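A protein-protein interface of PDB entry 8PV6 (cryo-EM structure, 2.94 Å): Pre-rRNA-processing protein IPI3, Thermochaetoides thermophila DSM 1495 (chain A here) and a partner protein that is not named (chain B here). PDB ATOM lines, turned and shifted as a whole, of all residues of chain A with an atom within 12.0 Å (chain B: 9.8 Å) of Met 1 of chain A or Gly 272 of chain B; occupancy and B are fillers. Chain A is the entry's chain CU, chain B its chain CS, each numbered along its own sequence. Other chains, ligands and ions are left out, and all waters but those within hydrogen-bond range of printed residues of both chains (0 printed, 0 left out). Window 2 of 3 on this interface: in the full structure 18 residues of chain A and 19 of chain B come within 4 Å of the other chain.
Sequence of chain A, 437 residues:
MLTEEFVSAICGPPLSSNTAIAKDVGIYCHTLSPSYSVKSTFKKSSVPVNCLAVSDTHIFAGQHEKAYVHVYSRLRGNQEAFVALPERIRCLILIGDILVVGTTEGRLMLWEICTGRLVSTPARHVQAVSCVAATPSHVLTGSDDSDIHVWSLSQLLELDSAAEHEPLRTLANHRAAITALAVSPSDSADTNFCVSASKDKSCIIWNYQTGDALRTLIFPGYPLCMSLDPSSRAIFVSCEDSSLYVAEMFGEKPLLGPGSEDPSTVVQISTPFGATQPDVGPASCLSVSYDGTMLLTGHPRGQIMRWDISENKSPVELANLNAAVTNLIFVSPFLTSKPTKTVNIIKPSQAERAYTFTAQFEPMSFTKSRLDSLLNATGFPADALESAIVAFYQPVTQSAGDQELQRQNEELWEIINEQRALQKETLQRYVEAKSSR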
ATOM      1  N   MET A   1      28.787  -9.626  -0.200  1.00  0.00           N
ATOM      2  CA  MET A   1      29.453  -9.810  -1.483  1.00  0.00           C
ATOM      3  C   MET A   1      28.655 -10.742  -2.386  1.00  0.00           C
ATOM      4  O   MET A   1      28.732 -11.963  -2.258  1.00  0.00           O
ATOM      5  CB  MET A   1      30.867 -10.357  -1.282  1.00  0.00           C
ATOM      6  CG  MET A   1      31.688 -10.433  -2.559  1.00  0.00           C
ATOM      7  SD  MET A   1      32.047  -8.807  -3.248  1.00  0.00           S
ATOM      8  CE  MET A   1      32.331  -9.219  -4.968  1.00  0.00           C
ATOM      9  N   LEU A   2      27.885 -10.158  -3.301  1.00  0.00           N
ATOM     10  CA  LEU A   2      27.099 -10.960  -4.226  1.00  0.00           C
ATOM     11  C   LEU A   2      27.832 -11.115  -5.550  1.00  0.00           C
ATOM     12  O   LEU A   2      28.336 -10.145  -6.120  1.00  0.00           O
ATOM     13  CB  LEU A   2      25.731 -10.320  -4.455  1.00  0.00           C
ATOM     14  CG  LEU A   2      24.967  -9.889  -3.208  1.00  0.00           C
ATOM     15  CD1 LEU A   2      23.691  -9.173  -3.605  1.00  0.00           C
ATOM     16  CD2 LEU A   2      24.665 -11.085  -2.329  1.00  0.00           C
ATOM     17  N   THR A   3      27.887 -12.350  -6.041  1.00  0.00           N
ATOM     18  CA  THR A   3      28.504 -12.664  -7.321  1.00  0.00           C
ATOM     19  C   THR A   3      27.420 -13.108  -8.290  1.00  0.00           C
ATOM     20  O   THR A   3      26.653 -14.027  -7.990  1.00  0.00           O
ATOM     21  CB  THR A   3      29.562 -13.760  -7.174  1.00  0.00           C
ATOM     22  OG1 THR A   3      28.945 -14.961  -6.694  1.00  0.00           O
ATOM     23  CG2 THR A   3      30.641 -13.329  -6.195  1.00  0.00           C
ATOM     24  N   GLU A   4      27.359 -12.455  -9.446  1.00  0.00           N
ATOM     25  CA  GLU A   4      26.380 -12.765 -10.475  1.00  0.00           C
ATOM     26  C   GLU A   4      27.031 -13.647 -11.530  1.00  0.00           C
ATOM     27  O   GLU A   4      28.155 -13.377 -11.958  1.00  0.00           O
ATOM     28  CB  GLU A   4      25.831 -11.487 -11.110  1.00  0.00           C
ATOM     29  CG  GLU A   4      24.572 -11.703 -11.924  1.00  0.00           C
ATOM     30  CD  GLU A   4      23.771 -10.433 -12.103  1.00  0.00           C
ATOM     31  OE1 GLU A   4      24.242  -9.363 -11.668  1.00  0.00           O
ATOM     32  OE2 GLU A   4      22.662 -10.509 -12.671  1.00  0.00           O
ATOM     33  N   GLU A   5      26.330 -14.701 -11.939  1.00  0.00           N
ATOM     34  CA  GLU A   5      26.866 -15.676 -12.877  1.00  0.00           C
ATOM     35  C   GLU A   5      25.870 -15.913 -14.001  1.00  0.00           C
ATOM     36  O   GLU A   5      24.676 -15.636 -13.861  1.00  0.00           O
ATOM     37  CB  GLU A   5      27.186 -17.004 -12.181  1.00  0.00           C
ATOM     38  CG  GLU A   5      28.249 -16.903 -11.098  1.00  0.00           C
ATOM     39  CD  GLU A   5      28.618 -18.251 -10.515  1.00  0.00           C
ATOM     40  OE1 GLU A   5      28.160 -19.279 -11.055  1.00  0.00           O
ATOM     41  OE2 GLU A   5      29.365 -18.283  -9.515  1.00  0.00           O
ATOM     42  N   THR A  31      31.270 -15.829 -14.588  1.00  0.00           N
ATOM     43  CA  THR A  31      30.898 -14.874 -13.552  1.00  0.00           C
ATOM     44  C   THR A  31      30.979 -13.472 -14.141  1.00  0.00           C
ATOM     45  O   THR A  31      32.061 -13.024 -14.535  1.00  0.00           O
ATOM     46  CB  THR A  31      31.813 -14.992 -12.333  1.00  0.00           C
ATOM     47  OG1 THR A  31      33.032 -14.282 -12.580  1.00  0.00           O
ATOM     48  CG2 THR A  31      32.137 -16.448 -12.048  1.00  0.00           C
ATOM     49  N   LEU A  32      29.837 -12.786 -14.202  1.00  0.00           N
ATOM     50  CA  LEU A  32      29.805 -11.439 -14.762  1.00  0.00           C
ATOM     51  C   LEU A  32      30.437 -10.425 -13.816  1.00  0.00           C
ATOM     52  O   LEU A  32      31.212  -9.564 -14.249  1.00  0.00           O
ATOM     53  CB  LEU A  32      28.365 -11.041 -15.077  1.00  0.00           C
ATOM     54  CG  LEU A  32      28.159  -9.645 -15.663  1.00  0.00           C
ATOM     55  CD1 LEU A  32      28.828  -9.535 -17.020  1.00  0.00           C
ATOM     56  CD2 LEU A  32      26.679  -9.317 -15.760  1.00  0.00           C
ATOM     57  N   SER A  33      30.119 -10.508 -12.526  1.00  0.00           N
ATOM     58  CA  SER A  33      30.572  -9.536 -11.546  1.00  0.00           C
ATOM     59  C   SER A  33      31.366 -10.253 -10.459  1.00  0.00           C
ATOM     60  O   SER A  33      31.001 -11.375 -10.066  1.00  0.00           O
ATOM     61  CB  SER A  33      29.382  -8.787 -10.932  1.00  0.00           C
ATOM     62  OG  SER A  33      28.620  -9.643 -10.100  1.00  0.00           O
ATOM     63  N   PRO A  34      32.447  -9.649  -9.938  1.00  0.00           N
ATOM     64  CA  PRO A  34      32.977  -8.337 -10.325  1.00  0.00           C
ATOM     65  C   PRO A  34      33.894  -8.376 -11.547  1.00  0.00           C
ATOM     66  O   PRO A  34      34.047  -7.361 -12.226  1.00  0.00           O
ATOM     67  CB  PRO A  34      33.758  -7.902  -9.085  1.00  0.00           C
ATOM     68  CG  PRO A  34      34.201  -9.174  -8.460  1.00  0.00           C
ATOM     69  CD  PRO A  34      33.170 -10.220  -8.788  1.00  0.00           C
ATOM     70  N   SER A  35      34.491  -9.533 -11.823  1.00  0.00           N
ATOM     71  CA  SER A  35      35.426  -9.693 -12.926  1.00  0.00           C
ATOM     72  C   SER A  35      34.963 -10.829 -13.823  1.00  0.00           C
ATOM     73  O   SER A  35      34.517 -11.871 -13.334  1.00  0.00           O
ATOM     74  CB  SER A  35      36.842  -9.969 -12.413  1.00  0.00           C
ATOM     75  OG  SER A  35      36.869 -11.126 -11.595  1.00  0.00           O
ATOM     76  N   TYR A  36      35.072 -10.623 -15.132  1.00  0.00           N
ATOM     77  CA  TYR A  36      34.690 -11.654 -16.086  1.00  0.00           C
ATOM     78  C   TYR A  36      35.723 -12.773 -16.114  1.00  0.00           C
ATOM     79  O   TYR A  36      36.924 -12.529 -16.258  1.00  0.00           O
ATOM     80  CB  TYR A  36      34.535 -11.043 -17.476  1.00  0.00           C
ATOM     81  CG  TYR A  36      34.129 -12.030 -18.539  1.00  0.00           C
ATOM     82  CD1 TYR A  36      32.820 -12.481 -18.633  1.00  0.00           C
ATOM     83  CD2 TYR A  36      35.055 -12.510 -19.452  1.00  0.00           C
ATOM     84  CE1 TYR A  36      32.447 -13.382 -19.611  1.00  0.00           C
ATOM     85  CE2 TYR A  36      34.694 -13.413 -20.425  1.00  0.00           C
ATOM     86  CZ  TYR A  36      33.388 -13.843 -20.505  1.00  0.00           C
ATOM     87  OH  TYR A  36      33.026 -14.741 -21.481  1.00  0.00           O
ATOM     88  N   SER A  37      35.246 -14.008 -15.983  1.00  0.00           N
ATOM     89  CA  SER A  37      36.108 -15.179 -16.034  1.00  0.00           C
ATOM     90  C   SER A  37      35.265 -16.381 -16.426  1.00  0.00           C
ATOM     91  O   SER A  37      34.038 -16.362 -16.308  1.00  0.00           O
ATOM     92  CB  SER A  37      36.807 -15.426 -14.694  1.00  0.00           C
ATOM     93  OG  SER A  37      35.862 -15.598 -13.653  1.00  0.00           O
ATOM     94  N   LYS A  39      34.230 -19.651 -15.327  1.00  0.00           N
ATOM     95  CA  LYS A  39      34.222 -20.412 -14.082  1.00  0.00           C
ATOM     96  C   LYS A  39      34.223 -21.915 -14.342  1.00  0.00           C
ATOM     97  O   LYS A  39      34.976 -22.657 -13.701  1.00  0.00           O
ATOM     98  CB  LYS A  39      33.021 -20.017 -13.225  1.00  0.00           C
ATOM     99  CG  LYS A  39      33.066 -20.576 -11.815  1.00  0.00           C
ATOM    100  CD  LYS A  39      31.936 -20.026 -10.964  1.00  0.00           C
ATOM    101  CE  LYS A  39      32.072 -20.470  -9.518  1.00  0.00           C
ATOM    102  NZ  LYS A  39      31.004 -19.892  -8.658  1.00  0.00           N
ATOM    103  N   TYR A 290      20.157  -9.490 -12.806  1.00  0.00           N
ATOM    104  CA  TYR A 290      19.300  -9.509 -11.624  1.00  0.00           C
ATOM    105  C   TYR A 290      18.919  -8.101 -11.192  1.00  0.00           C
ATOM    106  O   TYR A 290      17.775  -7.852 -10.796  1.00  0.00           O
ATOM    107  CB  TYR A 290      20.009 -10.246 -10.487  1.00  0.00           C
ATOM    108  CG  TYR A 290      19.132 -10.587  -9.301  1.00  0.00           C
ATOM    109  CD1 TYR A 290      19.064  -9.746  -8.198  1.00  0.00           C
ATOM    110  CD2 TYR A 290      18.384 -11.756  -9.281  1.00  0.00           C
ATOM    111  CE1 TYR A 290      18.273 -10.058  -7.112  1.00  0.00           C
ATOM    112  CE2 TYR A 290      17.591 -12.077  -8.199  1.00  0.00           C
ATOM    113  CZ  TYR A 290      17.539 -11.223  -7.118  1.00  0.00           C
ATOM    114  OH  TYR A 290      16.747 -11.539  -6.039  1.00  0.00           O
ATOM    115  N   ASP A 291      19.870  -7.170 -11.246  1.00  0.00           N
ATOM    116  CA  ASP A 291      19.563  -5.775 -10.955  1.00  0.00           C
ATOM    117  C   ASP A 291      18.658  -5.182 -12.026  1.00  0.00           C
ATOM    118  O   ASP A 291      17.779  -4.366 -11.727  1.00  0.00           O
ATOM    119  CB  ASP A 291      20.859  -4.974 -10.844  1.00  0.00           C
ATOM    120  CG  ASP A 291      20.690  -3.701 -10.044  1.00  0.00           C
ATOM    121  OD1 ASP A 291      21.713  -3.053  -9.740  1.00  0.00           O
ATOM    122  OD2 ASP A 291      19.542  -3.358  -9.702  1.00  0.00           O
ATOM    123  N   THR A 293      20.057  -3.572 -14.686  1.00  0.00           N
ATOM    124  CA  THR A 293      20.785  -2.482 -15.323  1.00  0.00           C
ATOM    125  C   THR A 293      21.690  -2.993 -16.436  1.00  0.00           C
ATOM    126  O   THR A 293      21.928  -2.290 -17.425  1.00  0.00           O
ATOM    127  CB  THR A 293      21.598  -1.720 -14.281  1.00  0.00           C
ATOM    128  OG1 THR A 293      22.686  -2.537 -13.834  1.00  0.00           O
ATOM    129  CG2 THR A 293      20.725  -1.371 -13.092  1.00  0.00           C
ATOM    130  N   MET A 294      22.205  -4.212 -16.296  1.00  0.00           N
ATOM    131  CA  MET A 294      23.083  -4.809 -17.292  1.00  0.00           C
ATOM    132  C   MET A 294      22.287  -5.752 -18.180  1.00  0.00           C
ATOM    133  O   MET A 294      21.305  -6.361 -17.743  1.00  0.00           O
ATOM    134  CB  MET A 294      24.251  -5.563 -16.645  1.00  0.00           C
ATOM    135  CG  MET A 294      25.074  -4.732 -15.679  1.00  0.00           C
ATOM    136  SD  MET A 294      26.085  -5.743 -14.581  1.00  0.00           S
ATOM    137  CE  MET A 294      25.795  -4.936 -13.010  1.00  0.00           C
ATOM    138  N   ARG A 306      27.817  -6.732 -23.524  1.00  0.00           N
ATOM    139  CA  ARG A 306      27.168  -6.223 -22.326  1.00  0.00           C
ATOM    140  C   ARG A 306      26.681  -4.808 -22.594  1.00  0.00           C
ATOM    141  O   ARG A 306      27.424  -3.984 -23.136  1.00  0.00           O
ATOM    142  CB  ARG A 306      28.119  -6.237 -21.129  1.00  0.00           C
ATOM    143  CG  ARG A 306      27.443  -5.905 -19.811  1.00  0.00           C
ATOM    144  CD  ARG A 306      28.447  -5.812 -18.677  1.00  0.00           C
ATOM    145  NE  ARG A 306      29.498  -4.842 -18.953  1.00  0.00           N
ATOM    146  CZ  ARG A 306      30.532  -4.614 -18.155  1.00  0.00           C
ATOM    147  NH1 ARG A 306      30.680  -5.265 -17.014  1.00  0.00           N
ATOM    148  NH2 ARG A 306      31.440  -3.710 -18.511  1.00  0.00           N
ATOM    149  N   VAL A 331      21.921 -16.478 -13.519  1.00  0.00           N
ATOM    150  CA  VAL A 331      21.668 -17.207 -12.283  1.00  0.00           C
ATOM    151  C   VAL A 331      21.487 -16.183 -11.172  1.00  0.00           C
ATOM    152  O   VAL A 331      22.189 -15.167 -11.138  1.00  0.00           O
ATOM    153  CB  VAL A 331      22.816 -18.187 -11.950  1.00  0.00           C
ATOM    154  CG1 VAL A 331      22.438 -19.094 -10.788  1.00  0.00           C
ATOM    155  CG2 VAL A 331      23.185 -19.016 -13.166  1.00  0.00           C
ATOM    156  N   SER A 332      20.531 -16.437 -10.284  1.00  0.00           N
ATOM    157  CA  SER A 332      20.287 -15.526  -9.177  1.00  0.00           C
ATOM    158  C   SER A 332      21.472 -15.537  -8.216  1.00  0.00           C
ATOM    159  O   SER A 332      21.966 -16.611  -7.851  1.00  0.00           O
ATOM    160  CB  SER A 332      19.009 -15.914  -8.435  1.00  0.00           C
ATOM    161  OG  SER A 332      19.149 -17.180  -7.815  1.00  0.00           O
ATOM    162  N   PRO A 333      21.964 -14.366  -7.797  1.00  0.00           N
ATOM    163  CA  PRO A 333      23.080 -14.329  -6.839  1.00  0.00           C
ATOM    164  C   PRO A 333      22.724 -14.838  -5.455  1.00  0.00           C
ATOM    165  O   PRO A 333      23.638 -15.180  -4.692  1.00  0.00           O
ATOM    166  CB  PRO A 333      23.453 -12.843  -6.796  1.00  0.00           C
ATOM    167  CG  PRO A 333      22.211 -12.136  -7.203  1.00  0.00           C
ATOM    168  CD  PRO A 333      21.555 -13.017  -8.219  1.00  0.00           C
ATOM    169  N   PHE A 334      21.445 -14.904  -5.105  1.00  0.00           N
ATOM    170  CA  PHE A 334      21.012 -15.397  -3.809  1.00  0.00           C
ATOM    171  C   PHE A 334      20.693 -16.882  -3.899  1.00  0.00           C
ATOM    172  O   PHE A 334      20.368 -17.408  -4.967  1.00  0.00           O
ATOM    173  CB  PHE A 334      19.780 -14.639  -3.304  1.00  0.00           C
ATOM    174  CG  PHE A 334      20.038 -13.194  -3.009  1.00  0.00           C
ATOM    175  CD1 PHE A 334      20.698 -12.817  -1.855  1.00  0.00           C
ATOM    176  CD2 PHE A 334      19.610 -12.212  -3.882  1.00  0.00           C
ATOM    177  CE1 PHE A 334      20.932 -11.488  -1.581  1.00  0.00           C
ATOM    178  CE2 PHE A 334      19.840 -10.883  -3.614  1.00  0.00           C
ATOM    179  CZ  PHE A 334      20.501 -10.520  -2.463  1.00  0.00           C
ATOM    180  N   LEU A 335      20.792 -17.555  -2.759  1.00  0.00           N
ATOM    181  CA  LEU A 335      20.416 -18.956  -2.661  1.00  0.00           C
ATOM    182  C   LEU A 335      18.961 -19.062  -2.226  1.00  0.00           C
ATOM    183  O   LEU A 335      18.488 -18.281  -1.395  1.00  0.00           O
ATOM    184  CB  LEU A 335      21.325 -19.712  -1.685  1.00  0.00           C
ATOM    185  CG  LEU A 335      21.245 -19.533  -0.162  1.00  0.00           C
ATOM    186  CD1 LEU A 335      21.985 -20.669   0.525  1.00  0.00           C
ATOM    187  CD2 LEU A 335      21.806 -18.196   0.305  1.00  0.00           C
ATOM    188  N   PRO B 177      32.307   6.906  -5.883  1.00  0.00           N
ATOM    189  CA  PRO B 177      33.053   6.266  -4.787  1.00  0.00           C
ATOM    190  C   PRO B 177      34.561   6.433  -4.904  1.00  0.00           C
ATOM    191  O   PRO B 177      35.166   6.031  -5.901  1.00  0.00           O
ATOM    192  CB  PRO B 177      32.653   4.791  -4.906  1.00  0.00           C
ATOM    193  CG  PRO B 177      31.334   4.816  -5.571  1.00  0.00           C
ATOM    194  CD  PRO B 177      31.394   5.954  -6.541  1.00  0.00           C
ATOM    195  N   PHE B 265      22.084   2.237  -8.209  1.00  0.00           N
ATOM    196  CA  PHE B 265      22.365   1.280  -7.140  1.00  0.00           C
ATOM    197  C   PHE B 265      23.850   1.167  -6.821  1.00  0.00           C
ATOM    198  O   PHE B 265      24.299   0.128  -6.327  1.00  0.00           O
ATOM    199  CB  PHE B 265      21.792  -0.105  -7.460  1.00  0.00           C
ATOM    200  CG  PHE B 265      20.369  -0.070  -7.923  1.00  0.00           C
ATOM    201  CD1 PHE B 265      19.345   0.175  -7.030  1.00  0.00           C
ATOM    202  CD2 PHE B 265      20.056  -0.269  -9.255  1.00  0.00           C
ATOM    203  CE1 PHE B 265      18.039   0.215  -7.453  1.00  0.00           C
ATOM    204  CE2 PHE B 265      18.746  -0.232  -9.684  1.00  0.00           C
ATOM    205  CZ  PHE B 265      17.738   0.011  -8.781  1.00  0.00           C
ATOM    206  N   ALA B 266      24.629   2.215  -7.096  1.00  0.00           N
ATOM    207  CA  ALA B 266      26.034   2.208  -6.710  1.00  0.00           C
ATOM    208  C   ALA B 266      26.200   2.432  -5.215  1.00  0.00           C
ATOM    209  O   ALA B 266      27.213   2.028  -4.636  1.00  0.00           O
ATOM    210  CB  ALA B 266      26.804   3.269  -7.497  1.00  0.00           C
ATOM    211  N   TYR B 267      25.221   3.077  -4.577  1.00  0.00           N
ATOM    212  CA  TYR B 267      25.281   3.287  -3.137  1.00  0.00           C
ATOM    213  C   TYR B 267      25.017   2.006  -2.360  1.00  0.00           C
ATOM    214  O   TYR B 267      25.412   1.911  -1.193  1.00  0.00           O
ATOM    215  CB  TYR B 267      24.290   4.377  -2.713  1.00  0.00           C
ATOM    216  CG  TYR B 267      22.850   4.150  -3.132  1.00  0.00           C
ATOM    217  CD1 TYR B 267      22.401   4.535  -4.389  1.00  0.00           C
ATOM    218  CD2 TYR B 267      21.938   3.566  -2.263  1.00  0.00           C
ATOM    219  CE1 TYR B 267      21.091   4.334  -4.773  1.00  0.00           C
ATOM    220  CE2 TYR B 267      20.623   3.363  -2.639  1.00  0.00           C
ATOM    221  CZ  TYR B 267      20.208   3.747  -3.894  1.00  0.00           C
ATOM    222  OH  TYR B 267      18.900   3.546  -4.272  1.00  0.00           O
ATOM    223  N   LEU B 268      24.354   1.026  -2.972  1.00  0.00           N
ATOM    224  CA  LEU B 268      24.113  -0.243  -2.296  1.00  0.00           C
ATOM    225  C   LEU B 268      25.390  -1.059  -2.155  1.00  0.00           C
ATOM    226  O   LEU B 268      25.608  -1.687  -1.111  1.00  0.00           O
ATOM    227  CB  LEU B 268      23.053  -1.045  -3.046  1.00  0.00           C
ATOM    228  CG  LEU B 268      21.699  -0.356  -3.172  1.00  0.00           C
ATOM    229  CD1 LEU B 268      20.732  -1.211  -3.961  1.00  0.00           C
ATOM    230  CD2 LEU B 268      21.159  -0.079  -1.792  1.00  0.00           C
ATOM    231  N   ASN B 269      26.238  -1.048  -3.192  1.00  0.00           N
ATOM    232  CA  ASN B 269      27.487  -1.817  -3.247  1.00  0.00           C
ATOM    233  C   ASN B 269      27.236  -3.305  -3.013  1.00  0.00           C
ATOM    234  O   ASN B 269      27.961  -3.972  -2.273  1.00  0.00           O
ATOM    235  CB  ASN B 269      28.522  -1.271  -2.259  1.00  0.00           C
ATOM    236  CG  ASN B 269      29.939  -1.654  -2.627  1.00  0.00           C
ATOM    237  OD1 ASN B 269      30.275  -1.777  -3.805  1.00  0.00           O
ATOM    238  ND2 ASN B 269      30.779  -1.849  -1.619  1.00  0.00           N
ATOM    239  N   LEU B 270      26.181  -3.828  -3.641  1.00  0.00           N
ATOM    240  CA  LEU B 270      25.838  -5.232  -3.456  1.00  0.00           C
ATOM    241  C   LEU B 270      26.800  -6.144  -4.206  1.00  0.00           C
ATOM    242  O   LEU B 270      27.232  -7.173  -3.674  1.00  0.00           O
ATOM    243  CB  LEU B 270      24.400  -5.483  -3.905  1.00  0.00           C
ATOM    244  CG  LEU B 270      23.302  -4.772  -3.115  1.00  0.00           C
ATOM    245  CD1 LEU B 270      21.956  -4.963  -3.782  1.00  0.00           C
ATOM    246  CD2 LEU B 270      23.265  -5.270  -1.683  1.00  0.00           C
ATOM    247  N   PHE B 271      27.150  -5.785  -5.439  1.00  0.00           N
ATOM    248  CA  PHE B 271      27.979  -6.625  -6.289  1.00  0.00           C
ATOM    249  C   PHE B 271      29.439  -6.193  -6.310  1.00  0.00           C
ATOM    250  O   PHE B 271      30.228  -6.753  -7.076  1.00  0.00           O
ATOM    251  CB  PHE B 271      27.418  -6.639  -7.712  1.00  0.00           C
ATOM    252  CG  PHE B 271      26.083  -7.312  -7.825  1.00  0.00           C
ATOM    253  CD1 PHE B 271      25.992  -8.692  -7.887  1.00  0.00           C
ATOM    254  CD2 PHE B 271      24.918  -6.566  -7.861  1.00  0.00           C
ATOM    255  CE1 PHE B 271      24.764  -9.314  -7.987  1.00  0.00           C
ATOM    256  CE2 PHE B 271      23.685  -7.183  -7.962  1.00  0.00           C
ATOM    257  CZ  PHE B 271      23.609  -8.557  -8.024  1.00  0.00           C
ATOM    258  N   GLY B 272      29.818  -5.217  -5.487  1.00  0.00           N
ATOM    259  CA  GLY B 272      31.173  -4.724  -5.437  1.00  0.00           C
ATOM    260  C   GLY B 272      31.871  -5.055  -4.127  1.00  0.00           C
ATOM    261  O   GLY B 272      31.305  -5.638  -3.206  1.00  0.00           O
ATOM    262  N   LEU B 273      33.139  -4.663  -4.070  1.00  0.00           N
ATOM    263  CA  LEU B 273      33.961  -4.872  -2.891  1.00  0.00           C
ATOM    264  C   LEU B 273      33.491  -3.981  -1.746  1.00  0.00           C
ATOM    265  O   LEU B 273      32.902  -2.921  -1.977  1.00  0.00           O
ATOM    266  CB  LEU B 273      35.428  -4.584  -3.205  1.00  0.00           C
ATOM    267  CG  LEU B 273      36.324  -5.648  -3.860  1.00  0.00           C
ATOM    268  CD1 LEU B 273      36.480  -6.851  -2.938  1.00  0.00           C
ATOM    269  CD2 LEU B 273      35.861  -6.077  -5.251  1.00  0.00           C
ATOM    270  N   PRO B 274      33.705  -4.409  -0.500  1.00  0.00           N
ATOM    271  CA  PRO B 274      33.436  -3.523   0.639  1.00  0.00           C
ATOM    272  C   PRO B 274      34.308  -2.277   0.586  1.00  0.00           C
ATOM    273  O   PRO B 274      35.472  -2.326   0.182  1.00  0.00           O
ATOM    274  CB  PRO B 274      33.772  -4.394   1.853  1.00  0.00           C
ATOM    275  CG  PRO B 274      33.587  -5.789   1.373  1.00  0.00           C
ATOM    276  CD  PRO B 274      34.007  -5.784  -0.068  1.00  0.00           C
ATOM    277  N   ARG B 275      33.732  -1.154   0.997  1.00  0.00           N
ATOM    278  CA  ARG B 275      34.367   0.150   0.867  1.00  0.00           C
ATOM    279  C   ARG B 275      34.856   0.631   2.224  1.00  0.00           C
ATOM    280  O   ARG B 275      34.120   0.570   3.214  1.00  0.00           O
ATOM    281  CB  ARG B 275      33.397   1.170   0.269  1.00  0.00           C
ATOM    282  CG  ARG B 275      32.915   0.831  -1.128  1.00  0.00           C
ATOM    283  CD  ARG B 275      31.853   1.813  -1.587  1.00  0.00           C
ATOM    284  NE  ARG B 275      31.232   1.406  -2.841  1.00  0.00           N
ATOM    285  CZ  ARG B 275      30.175   2.000  -3.378  1.00  0.00           C
ATOM    286  NH1 ARG B 275      29.593   3.033  -2.794  1.00  0.00           N
ATOM    287  NH2 ARG B 275      29.692   1.545  -4.530  1.00  0.00           N
ATOM    288  N   SER B 279      37.237   4.952   0.146  1.00  0.00           N
ATOM    289  CA  SER B 279      36.484   4.478  -1.007  1.00  0.00           C
ATOM    290  C   SER B 279      34.979   4.668  -0.869  1.00  0.00           C
ATOM    291  O   SER B 279      34.237   4.256  -1.766  1.00  0.00           O
ATOM    292  CB  SER B 279      36.784   2.997  -1.260  1.00  0.00           C
ATOM    293  OG  SER B 279      35.963   2.483  -2.293  1.00  0.00           O
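The backbone NH (N) of Leu 2 of chain A lies within hydrogen-bond range of the backbone carbonyl oxygen (O) of Leu 270 of chain B.
O of Gly 272 of chain B sits close to SD of Met 1 of chain A (3.3 Å).
O of Glu 4 of chain A is in hydrogen-bond range of N of Leu 32 of chain A.
N of Glu 4 of chain A sits at hydrogen-bond distance from OG of Ser 33 of chain A, at 3.2 Å.
OE2 of Glu 4 of chain A is in hydrogen-bond range of N of Tyr 290 of chain A (2.7 Å).
Among the printed residues, pairs that only touch across the chains: Met 1 of chain A with Phe 271 of chain B, Leu 2 of chain A with Phe 271 of chain B, Glu 4 of chain A with Phe 271 of chain B, Ser 33 of chain A with Phe 271 of chain B, Asp 291 of chain A with Phe 265 of chain B and Pro 333 of chain A with Phe 271 of chain B.
Met 1 of chain A touches just these residues of chain B: Phe 271 (3.9 Å) and Gly 272 (3.3 Å).
Leu 2 of chain A touches two residues of chain B.
Printed residues of chain B within 4 Å of Ser 33 of chain A: Phe 271 (3.6 Å).
Of the printed residues of chain A, Phe 265 of chain B touches Asp 291 (3.2 Å).
No residue of chain A comes within 4 Å of Asn 269 of chain B.
Phe 271 of chain B touches just these residues of chain A: Met 1 (3.9 Å), Leu 2 (3.3 Å), Glu 4 (3.7 Å), Ser 33 (3.6 Å) and Pro 333 (3.9 Å).
Gly 272 of chain B touches just one residue of chain A: Met 1.
No residue of chain A comes within 4 Å of Leu 273 of chain B.
No residue of chain A comes within 4 Å of Pro 274 of chain B.
The nearest residue of chain B that does not touch Met 1 of chain A is Leu 270 of chain B (4.1 Å).
The nearest printed residue of chain A that does not touch Leu 270 of chain B is Met 1 of chain A (4.1 Å).
Hydrophobic or aromatic side chains of chain A within 4 Å of the printed part of chain B: Met 1, Leu 2 and Pro 333.
Hydrophobic or aromatic side chains of chain B within 4 Å of the printed part of chain A: Phe 265, Leu 270 and Phe 271.
Among the printed residues, 8 pairs touch across the chains.
Among the printed residues, no Asp or Glu carboxylate lies within 4 Å of a Lys or Arg side-chain nitrogen of the other chain.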
